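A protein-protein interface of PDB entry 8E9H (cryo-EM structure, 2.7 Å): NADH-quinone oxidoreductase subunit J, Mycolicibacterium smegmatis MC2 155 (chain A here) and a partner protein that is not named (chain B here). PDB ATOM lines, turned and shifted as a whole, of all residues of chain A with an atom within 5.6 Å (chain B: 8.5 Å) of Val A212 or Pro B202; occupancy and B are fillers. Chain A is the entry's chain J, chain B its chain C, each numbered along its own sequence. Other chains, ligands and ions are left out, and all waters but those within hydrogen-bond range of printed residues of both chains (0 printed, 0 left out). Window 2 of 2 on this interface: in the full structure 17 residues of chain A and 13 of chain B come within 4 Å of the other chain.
The side-chain carboxylate (OD1) of Asp B203 is in hydrogen-bond range of the backbone NH (N) of Val A212.
The backbone NH (N) of Gly A211 is in hydrogen-bond range of the backbone carbonyl oxygen (O) of Val A221.
Asp B203 touches Gly A211 (OD1 to CA, 3.2 Å).
Val A212 touches Pro B202.
Asp B204 touches Val A212.
Tyr A213 touches Asp B203 (CZ to CB, 3.7 Å).
Tyr A213 touches Asp B204 (CD2 to CB, 3.8 Å).
Val A212 touches three residues of chain B.
Printed residues of chain B within 4 Å of Tyr A213: Asp B203 (3.7 Å) and Asp B204 (3.8 Å).
Pro B202 touches one residue of chain A.
Printed residues of chain A within 4 Å of Asp B203: Gly A211, Val A212 and Tyr A213.
Of the printed residues of chain A, Asp B204 touches Val A212 and Tyr A213.
The nearest residue of chain B that does not touch Val A212 is Met B201 (5.5 Å).
The nearest residue of chain A that does not touch Pro B202 is Tyr A213 (5.1 Å).
Of the 9 printed residues of chain A, 3 touch a printed residue of chain B.
Along chain A the printed residues that touch a printed residue of chain B span positions 211 to 213.
Of the 15 printed residues of chain B, 3 touch a printed residue of chain A.
Among the printed residues, 6 pairs touch across the chains.
Among the printed residues, no Asp or Glu carboxylate lies within 4 Å of a Lys or Arg side-chain nitrogen of the other chain.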
ATOM      1  N   ASN A 209      -9.188   9.034  10.315  1.00  0.00           N
ATOM      2  CA  ASN A 209      -9.300   8.523   8.966  1.00  0.00           C
ATOM      3  C   ASN A 209      -8.490   7.242   8.830  1.00  0.00           C
ATOM      4  O   ASN A 209      -7.537   7.015   9.574  1.00  0.00           O
ATOM      5  CB  ASN A 209      -8.802   9.564   7.969  1.00  0.00           C
ATOM      6  CG  ASN A 209      -7.356   9.949   8.212  1.00  0.00           C
ATOM      7  OD1 ASN A 209      -6.717   9.442   9.132  1.00  0.00           O
ATOM      8  ND2 ASN A 209      -6.832  10.844   7.390  1.00  0.00           N
ATOM      9  N   PRO A 210      -8.849   6.375   7.890  1.00  0.00           N
ATOM     10  CA  PRO A 210      -7.987   5.233   7.589  1.00  0.00           C
ATOM     11  C   PRO A 210      -6.649   5.700   7.047  1.00  0.00           C
ATOM     12  O   PRO A 210      -6.542   6.719   6.364  1.00  0.00           O
ATOM     13  CB  PRO A 210      -8.777   4.452   6.538  1.00  0.00           C
ATOM     14  CG  PRO A 210      -9.688   5.446   5.935  1.00  0.00           C
ATOM     15  CD  PRO A 210     -10.040   6.401   7.028  1.00  0.00           C
ATOM     16  N   GLY A 211      -5.613   4.933   7.370  1.00  0.00           N
ATOM     17  CA  GLY A 211      -4.262   5.284   6.978  1.00  0.00           C
ATOM     18  C   GLY A 211      -4.120   5.342   5.467  1.00  0.00           C
ATOM     19  O   GLY A 211      -4.701   4.540   4.742  1.00  0.00           O
ATOM     20  N   VAL A 212      -3.344   6.315   5.003  1.00  0.00           N
ATOM     21  CA  VAL A 212      -3.044   6.482   3.589  1.00  0.00           C
ATOM     22  C   VAL A 212      -1.564   6.194   3.408  1.00  0.00           C
ATOM     23  O   VAL A 212      -0.712   6.997   3.807  1.00  0.00           O
ATOM     24  CB  VAL A 212      -3.400   7.885   3.087  1.00  0.00           C
ATOM     25  CG1 VAL A 212      -2.972   8.047   1.646  1.00  0.00           C
ATOM     26  CG2 VAL A 212      -4.886   8.128   3.225  1.00  0.00           C
ATOM     27  N   TYR A 213      -1.255   5.051   2.813  1.00  0.00           N
ATOM     28  CA  TYR A 213       0.111   4.658   2.519  1.00  0.00           C
ATOM     29  C   TYR A 213       0.302   4.622   1.015  1.00  0.00           C
ATOM     30  O   TYR A 213      -0.655   4.423   0.264  1.00  0.00           O
ATOM     31  CB  TYR A 213       0.437   3.282   3.100  1.00  0.00           C
ATOM     32  CG  TYR A 213       0.219   3.163   4.585  1.00  0.00           C
ATOM     33  CD1 TYR A 213      -1.054   3.183   5.123  1.00  0.00           C
ATOM     34  CD2 TYR A 213       1.290   3.019   5.449  1.00  0.00           C
ATOM     35  CE1 TYR A 213      -1.256   3.072   6.476  1.00  0.00           C
ATOM     36  CE2 TYR A 213       1.096   2.909   6.805  1.00  0.00           C
ATOM     37  CZ  TYR A 213      -0.180   2.934   7.314  1.00  0.00           C
ATOM     38  OH  TYR A 213      -0.383   2.823   8.667  1.00  0.00           O
ATOM     39  N   ALA A 214       1.537   4.825   0.571  1.00  0.00           N
ATOM     40  CA  ALA A 214       1.857   4.511  -0.807  1.00  0.00           C
ATOM     41  C   ALA A 214       1.563   3.041  -1.052  1.00  0.00           C
ATOM     42  O   ALA A 214       1.977   2.174  -0.279  1.00  0.00           O
ATOM     43  CB  ALA A 214       3.324   4.817  -1.101  1.00  0.00           C
ATOM     44  N   HIS A 216      -1.356   1.781  -0.822  1.00  0.00           N
ATOM     45  CA  HIS A 216      -2.520   1.369  -0.040  1.00  0.00           C
ATOM     46  C   HIS A 216      -3.212   2.605   0.502  1.00  0.00           C
ATOM     47  O   HIS A 216      -2.649   3.304   1.348  1.00  0.00           O
ATOM     48  CB  HIS A 216      -2.115   0.445   1.108  1.00  0.00           C
ATOM     49  CG  HIS A 216      -1.498  -0.841   0.663  1.00  0.00           C
ATOM     50  ND1 HIS A 216      -2.210  -1.815  -0.001  1.00  0.00           N
ATOM     51  CD2 HIS A 216      -0.238  -1.317   0.794  1.00  0.00           C
ATOM     52  CE1 HIS A 216      -1.413  -2.834  -0.267  1.00  0.00           C
ATOM     53  NE2 HIS A 216      -0.211  -2.558   0.205  1.00  0.00           N
ATOM     54  N   ASN A 217      -4.428   2.869   0.029  1.00  0.00           N
ATOM     55  CA  ASN A 217      -5.228   3.953   0.583  1.00  0.00           C
ATOM     56  C   ASN A 217      -6.690   3.564   0.759  1.00  0.00           C
ATOM     57  O   ASN A 217      -7.524   4.449   0.981  1.00  0.00           O
ATOM     58  CB  ASN A 217      -5.125   5.203  -0.294  1.00  0.00           C
ATOM     59  CG  ASN A 217      -5.555   4.950  -1.717  1.00  0.00           C
ATOM     60  OD1 ASN A 217      -6.304   4.019  -1.995  1.00  0.00           O
ATOM     61  ND2 ASN A 217      -5.088   5.789  -2.630  1.00  0.00           N
ATOM     62  N   VAL A 221      -7.272  -0.002   5.276  1.00  0.00           N
ATOM     63  CA  VAL A 221      -5.928   0.217   5.799  1.00  0.00           C
ATOM     64  C   VAL A 221      -6.013   0.929   7.144  1.00  0.00           C
ATOM     65  O   VAL A 221      -6.774   1.896   7.278  1.00  0.00           O
ATOM     66  CB  VAL A 221      -5.081   1.028   4.810  1.00  0.00           C
ATOM     67  CG1 VAL A 221      -3.689   1.219   5.353  1.00  0.00           C
ATOM     68  CG2 VAL A 221      -5.035   0.341   3.461  1.00  0.00           C
ATOM     69  N   TYR B 183       1.339  17.179  15.464  1.00  0.00           N
ATOM     70  CA  TYR B 183       2.183  15.994  15.515  1.00  0.00           C
ATOM     71  C   TYR B 183       2.732  15.672  14.138  1.00  0.00           C
ATOM     72  O   TYR B 183       3.914  15.344  13.984  1.00  0.00           O
ATOM     73  CB  TYR B 183       1.407  14.795  16.047  1.00  0.00           C
ATOM     74  CG  TYR B 183       2.052  13.501  15.626  1.00  0.00           C
ATOM     75  CD1 TYR B 183       3.295  13.140  16.112  1.00  0.00           C
ATOM     76  CD2 TYR B 183       1.437  12.661  14.713  1.00  0.00           C
ATOM     77  CE1 TYR B 183       3.899  11.973  15.720  1.00  0.00           C
ATOM     78  CE2 TYR B 183       2.035  11.487  14.316  1.00  0.00           C
ATOM     79  CZ  TYR B 183       3.267  11.149  14.823  1.00  0.00           C
ATOM     80  OH  TYR B 183       3.873   9.981  14.430  1.00  0.00           O
ATOM     81  N   ASP B 184       1.883  15.761  13.118  1.00  0.00           N
ATOM     82  CA  ASP B 184       2.320  15.447  11.766  1.00  0.00           C
ATOM     83  C   ASP B 184       3.449  16.367  11.336  1.00  0.00           C
ATOM     84  O   ASP B 184       4.444  15.923  10.754  1.00  0.00           O
ATOM     85  CB  ASP B 184       1.143  15.565  10.801  1.00  0.00           C
ATOM     86  CG  ASP B 184       1.418  14.903   9.473  1.00  0.00           C
ATOM     87  OD1 ASP B 184       2.546  14.411   9.279  1.00  0.00           O
ATOM     88  OD2 ASP B 184       0.510  14.880   8.619  1.00  0.00           O
ATOM     89  N   PHE B 185       3.317  17.655  11.626  1.00  0.00           N
ATOM     90  CA  PHE B 185       4.256  18.640  11.114  1.00  0.00           C
ATOM     91  C   PHE B 185       5.408  18.942  12.059  1.00  0.00           C
ATOM     92  O   PHE B 185       6.349  19.630  11.652  1.00  0.00           O
ATOM     93  CB  PHE B 185       3.513  19.936  10.798  1.00  0.00           C
ATOM     94  CG  PHE B 185       2.605  19.834   9.613  1.00  0.00           C
ATOM     95  CD1 PHE B 185       2.992  19.139   8.485  1.00  0.00           C
ATOM     96  CD2 PHE B 185       1.357  20.416   9.636  1.00  0.00           C
ATOM     97  CE1 PHE B 185       2.159  19.039   7.403  1.00  0.00           C
ATOM     98  CE2 PHE B 185       0.521  20.318   8.555  1.00  0.00           C
ATOM     99  CZ  PHE B 185       0.923  19.627   7.437  1.00  0.00           C
ATOM    100  N   THR B 197      -2.720  10.107  14.920  1.00  0.00           N
ATOM    101  CA  THR B 197      -2.265   9.691  13.607  1.00  0.00           C
ATOM    102  C   THR B 197      -2.062  10.903  12.706  1.00  0.00           C
ATOM    103  O   THR B 197      -2.663  11.962  12.900  1.00  0.00           O
ATOM    104  CB  THR B 197      -3.272   8.737  12.973  1.00  0.00           C
ATOM    105  OG1 THR B 197      -4.508   9.426  12.754  1.00  0.00           O
ATOM    106  CG2 THR B 197      -3.520   7.553  13.881  1.00  0.00           C
ATOM    107  N   ARG B 198      -1.206  10.735  11.705  1.00  0.00           N
ATOM    108  CA  ARG B 198      -0.991  11.795  10.737  1.00  0.00           C
ATOM    109  C   ARG B 198      -2.298  12.132  10.030  1.00  0.00           C
ATOM    110  O   ARG B 198      -3.119  11.261   9.736  1.00  0.00           O
ATOM    111  CB  ARG B 198       0.061  11.383   9.713  1.00  0.00           C
ATOM    112  CG  ARG B 198       1.465  11.341  10.264  1.00  0.00           C
ATOM    113  CD  ARG B 198       2.473  11.116   9.163  1.00  0.00           C
ATOM    114  NE  ARG B 198       3.824  10.966   9.688  1.00  0.00           N
ATOM    115  CZ  ARG B 198       4.726  11.937   9.744  1.00  0.00           C
ATOM    116  NH1 ARG B 198       4.459  13.158   9.314  1.00  0.00           N
ATOM    117  NH2 ARG B 198       5.927  11.676  10.247  1.00  0.00           N
ATOM    118  N   ILE B 199      -2.486  13.420   9.759  1.00  0.00           N
ATOM    119  CA  ILE B 199      -3.730  13.901   9.175  1.00  0.00           C
ATOM    120  C   ILE B 199      -3.453  14.522   7.816  1.00  0.00           C
ATOM    121  O   ILE B 199      -4.233  14.351   6.875  1.00  0.00           O
ATOM    122  CB  ILE B 199      -4.432  14.895  10.116  1.00  0.00           C
ATOM    123  CG1 ILE B 199      -5.734  15.384   9.488  1.00  0.00           C
ATOM    124  CG2 ILE B 199      -3.532  16.070  10.432  1.00  0.00           C
ATOM    125  CD1 ILE B 199      -6.674  16.012  10.477  1.00  0.00           C
ATOM    126  N   GLU B 200      -2.343  15.248   7.700  1.00  0.00           N
ATOM    127  CA  GLU B 200      -1.973  15.879   6.440  1.00  0.00           C
ATOM    128  C   GLU B 200      -1.072  14.983   5.597  1.00  0.00           C
ATOM    129  O   GLU B 200      -1.418  14.642   4.463  1.00  0.00           O
ATOM    130  CB  GLU B 200      -1.279  17.213   6.716  1.00  0.00           C
ATOM    131  CG  GLU B 200      -2.182  18.250   7.352  1.00  0.00           C
ATOM    132  CD  GLU B 200      -3.168  18.838   6.379  1.00  0.00           C
ATOM    133  OE1 GLU B 200      -3.172  18.412   5.209  1.00  0.00           O
ATOM    134  OE2 GLU B 200      -3.939  19.732   6.783  1.00  0.00           O
ATOM    135  N   MET B 201       0.077  14.596   6.133  1.00  0.00           N
ATOM    136  CA  MET B 201       0.990  13.707   5.438  1.00  0.00           C
ATOM    137  C   MET B 201       0.452  12.284   5.385  1.00  0.00           C
ATOM    138  O   MET B 201      -0.336  11.873   6.238  1.00  0.00           O
ATOM    139  CB  MET B 201       2.345  13.708   6.133  1.00  0.00           C
ATOM    140  CG  MET B 201       3.052  15.030   6.093  1.00  0.00           C
ATOM    141  SD  MET B 201       3.559  15.346   4.399  1.00  0.00           S
ATOM    142  CE  MET B 201       2.474  16.683   3.987  1.00  0.00           C
ATOM    143  N   PRO B 202       0.869  11.506   4.388  1.00  0.00           N
ATOM    144  CA  PRO B 202       0.552  10.079   4.402  1.00  0.00           C
ATOM    145  C   PRO B 202       1.126   9.419   5.642  1.00  0.00           C
ATOM    146  O   PRO B 202       2.193   9.790   6.131  1.00  0.00           O
ATOM    147  CB  PRO B 202       1.220   9.552   3.128  1.00  0.00           C
ATOM    148  CG  PRO B 202       1.372  10.734   2.263  1.00  0.00           C
ATOM    149  CD  PRO B 202       1.614  11.884   3.178  1.00  0.00           C
ATOM    150  N   ASP B 203       0.399   8.427   6.156  1.00  0.00           N
ATOM    151  CA  ASP B 203       0.886   7.713   7.327  1.00  0.00           C
ATOM    152  C   ASP B 203       2.252   7.103   7.068  1.00  0.00           C
ATOM    153  O   ASP B 203       3.029   6.892   8.006  1.00  0.00           O
ATOM    154  CB  ASP B 203      -0.108   6.629   7.729  1.00  0.00           C
ATOM    155  CG  ASP B 203      -1.422   7.199   8.196  1.00  0.00           C
ATOM    156  OD1 ASP B 203      -2.185   7.701   7.347  1.00  0.00           O
ATOM    157  OD2 ASP B 203      -1.689   7.154   9.413  1.00  0.00           O
ATOM    158  N   ASP B 204       2.567   6.825   5.805  1.00  0.00           N
ATOM    159  CA  ASP B 204       3.860   6.270   5.439  1.00  0.00           C
ATOM    160  C   ASP B 204       4.947   7.329   5.338  1.00  0.00           C
ATOM    161  O   ASP B 204       6.111   6.977   5.131  1.00  0.00           O
ATOM    162  CB  ASP B 204       3.730   5.534   4.107  1.00  0.00           C
ATOM    163  CG  ASP B 204       4.945   4.703   3.783  1.00  0.00           C
ATOM    164  OD1 ASP B 204       5.656   4.299   4.723  1.00  0.00           O
ATOM    165  OD2 ASP B 204       5.186   4.448   2.587  1.00  0.00           O
ATOM    166  N   TRP B 205       4.603   8.604   5.481  1.00  0.00           N
ATOM    167  CA  TRP B 205       5.580   9.665   5.304  1.00  0.00           C
ATOM    168  C   TRP B 205       6.677   9.573   6.352  1.00  0.00           C
ATOM    169  O   TRP B 205       6.454   9.140   7.485  1.00  0.00           O
ATOM    170  CB  TRP B 205       4.907  11.030   5.388  1.00  0.00           C
ATOM    171  CG  TRP B 205       5.703  12.116   4.757  1.00  0.00           C
ATOM    172  CD1 TRP B 205       6.513  13.009   5.386  1.00  0.00           C
ATOM    173  CD2 TRP B 205       5.771  12.426   3.363  1.00  0.00           C
ATOM    174  NE1 TRP B 205       7.080  13.858   4.473  1.00  0.00           N
ATOM    175  CE2 TRP B 205       6.639  13.520   3.222  1.00  0.00           C
ATOM    176  CE3 TRP B 205       5.180  11.884   2.222  1.00  0.00           C
ATOM    177  CZ2 TRP B 205       6.931  14.083   1.988  1.00  0.00           C
ATOM    178  CZ3 TRP B 205       5.469  12.443   1.000  1.00  0.00           C
ATOM    179  CH2 TRP B 205       6.336  13.530   0.891  1.00  0.00           C
ATOM    180  N   GLU B 206       7.875   9.992   5.961  1.00  0.00           N
ATOM    181  CA  GLU B 206       9.026  10.023   6.849  1.00  0.00           C
ATOM    182  C   GLU B 206       9.370  11.470   7.172  1.00  0.00           C
ATOM    183  O   GLU B 206       9.516  12.294   6.265  1.00  0.00           O
ATOM    184  CB  GLU B 206      10.225   9.325   6.208  1.00  0.00           C
ATOM    185  N   GLY B 207       9.503  11.771   8.460  1.00  0.00           N
ATOM    186  CA  GLY B 207       9.844  13.108   8.891  1.00  0.00           C
ATOM    187  C   GLY B 207       8.623  13.960   9.168  1.00  0.00           C
ATOM    188  O   GLY B 207       7.484  13.605   8.869  1.00  0.00           O
ATOM    189  N   PRO B 209       7.333  17.689   8.388  1.00  0.00           N
ATOM    190  CA  PRO B 209       7.794  18.720   7.446  1.00  0.00           C
ATOM    191  C   PRO B 209       8.089  20.080   8.051  1.00  0.00           C
ATOM    192  O   PRO B 209       9.079  20.707   7.661  1.00  0.00           O
ATOM    193  CB  PRO B 209       6.643  18.797   6.442  1.00  0.00           C
ATOM    194  CG  PRO B 209       6.001  17.482   6.498  1.00  0.00           C
ATOM    195  CD  PRO B 209       6.116  17.018   7.907  1.00  0.00           C
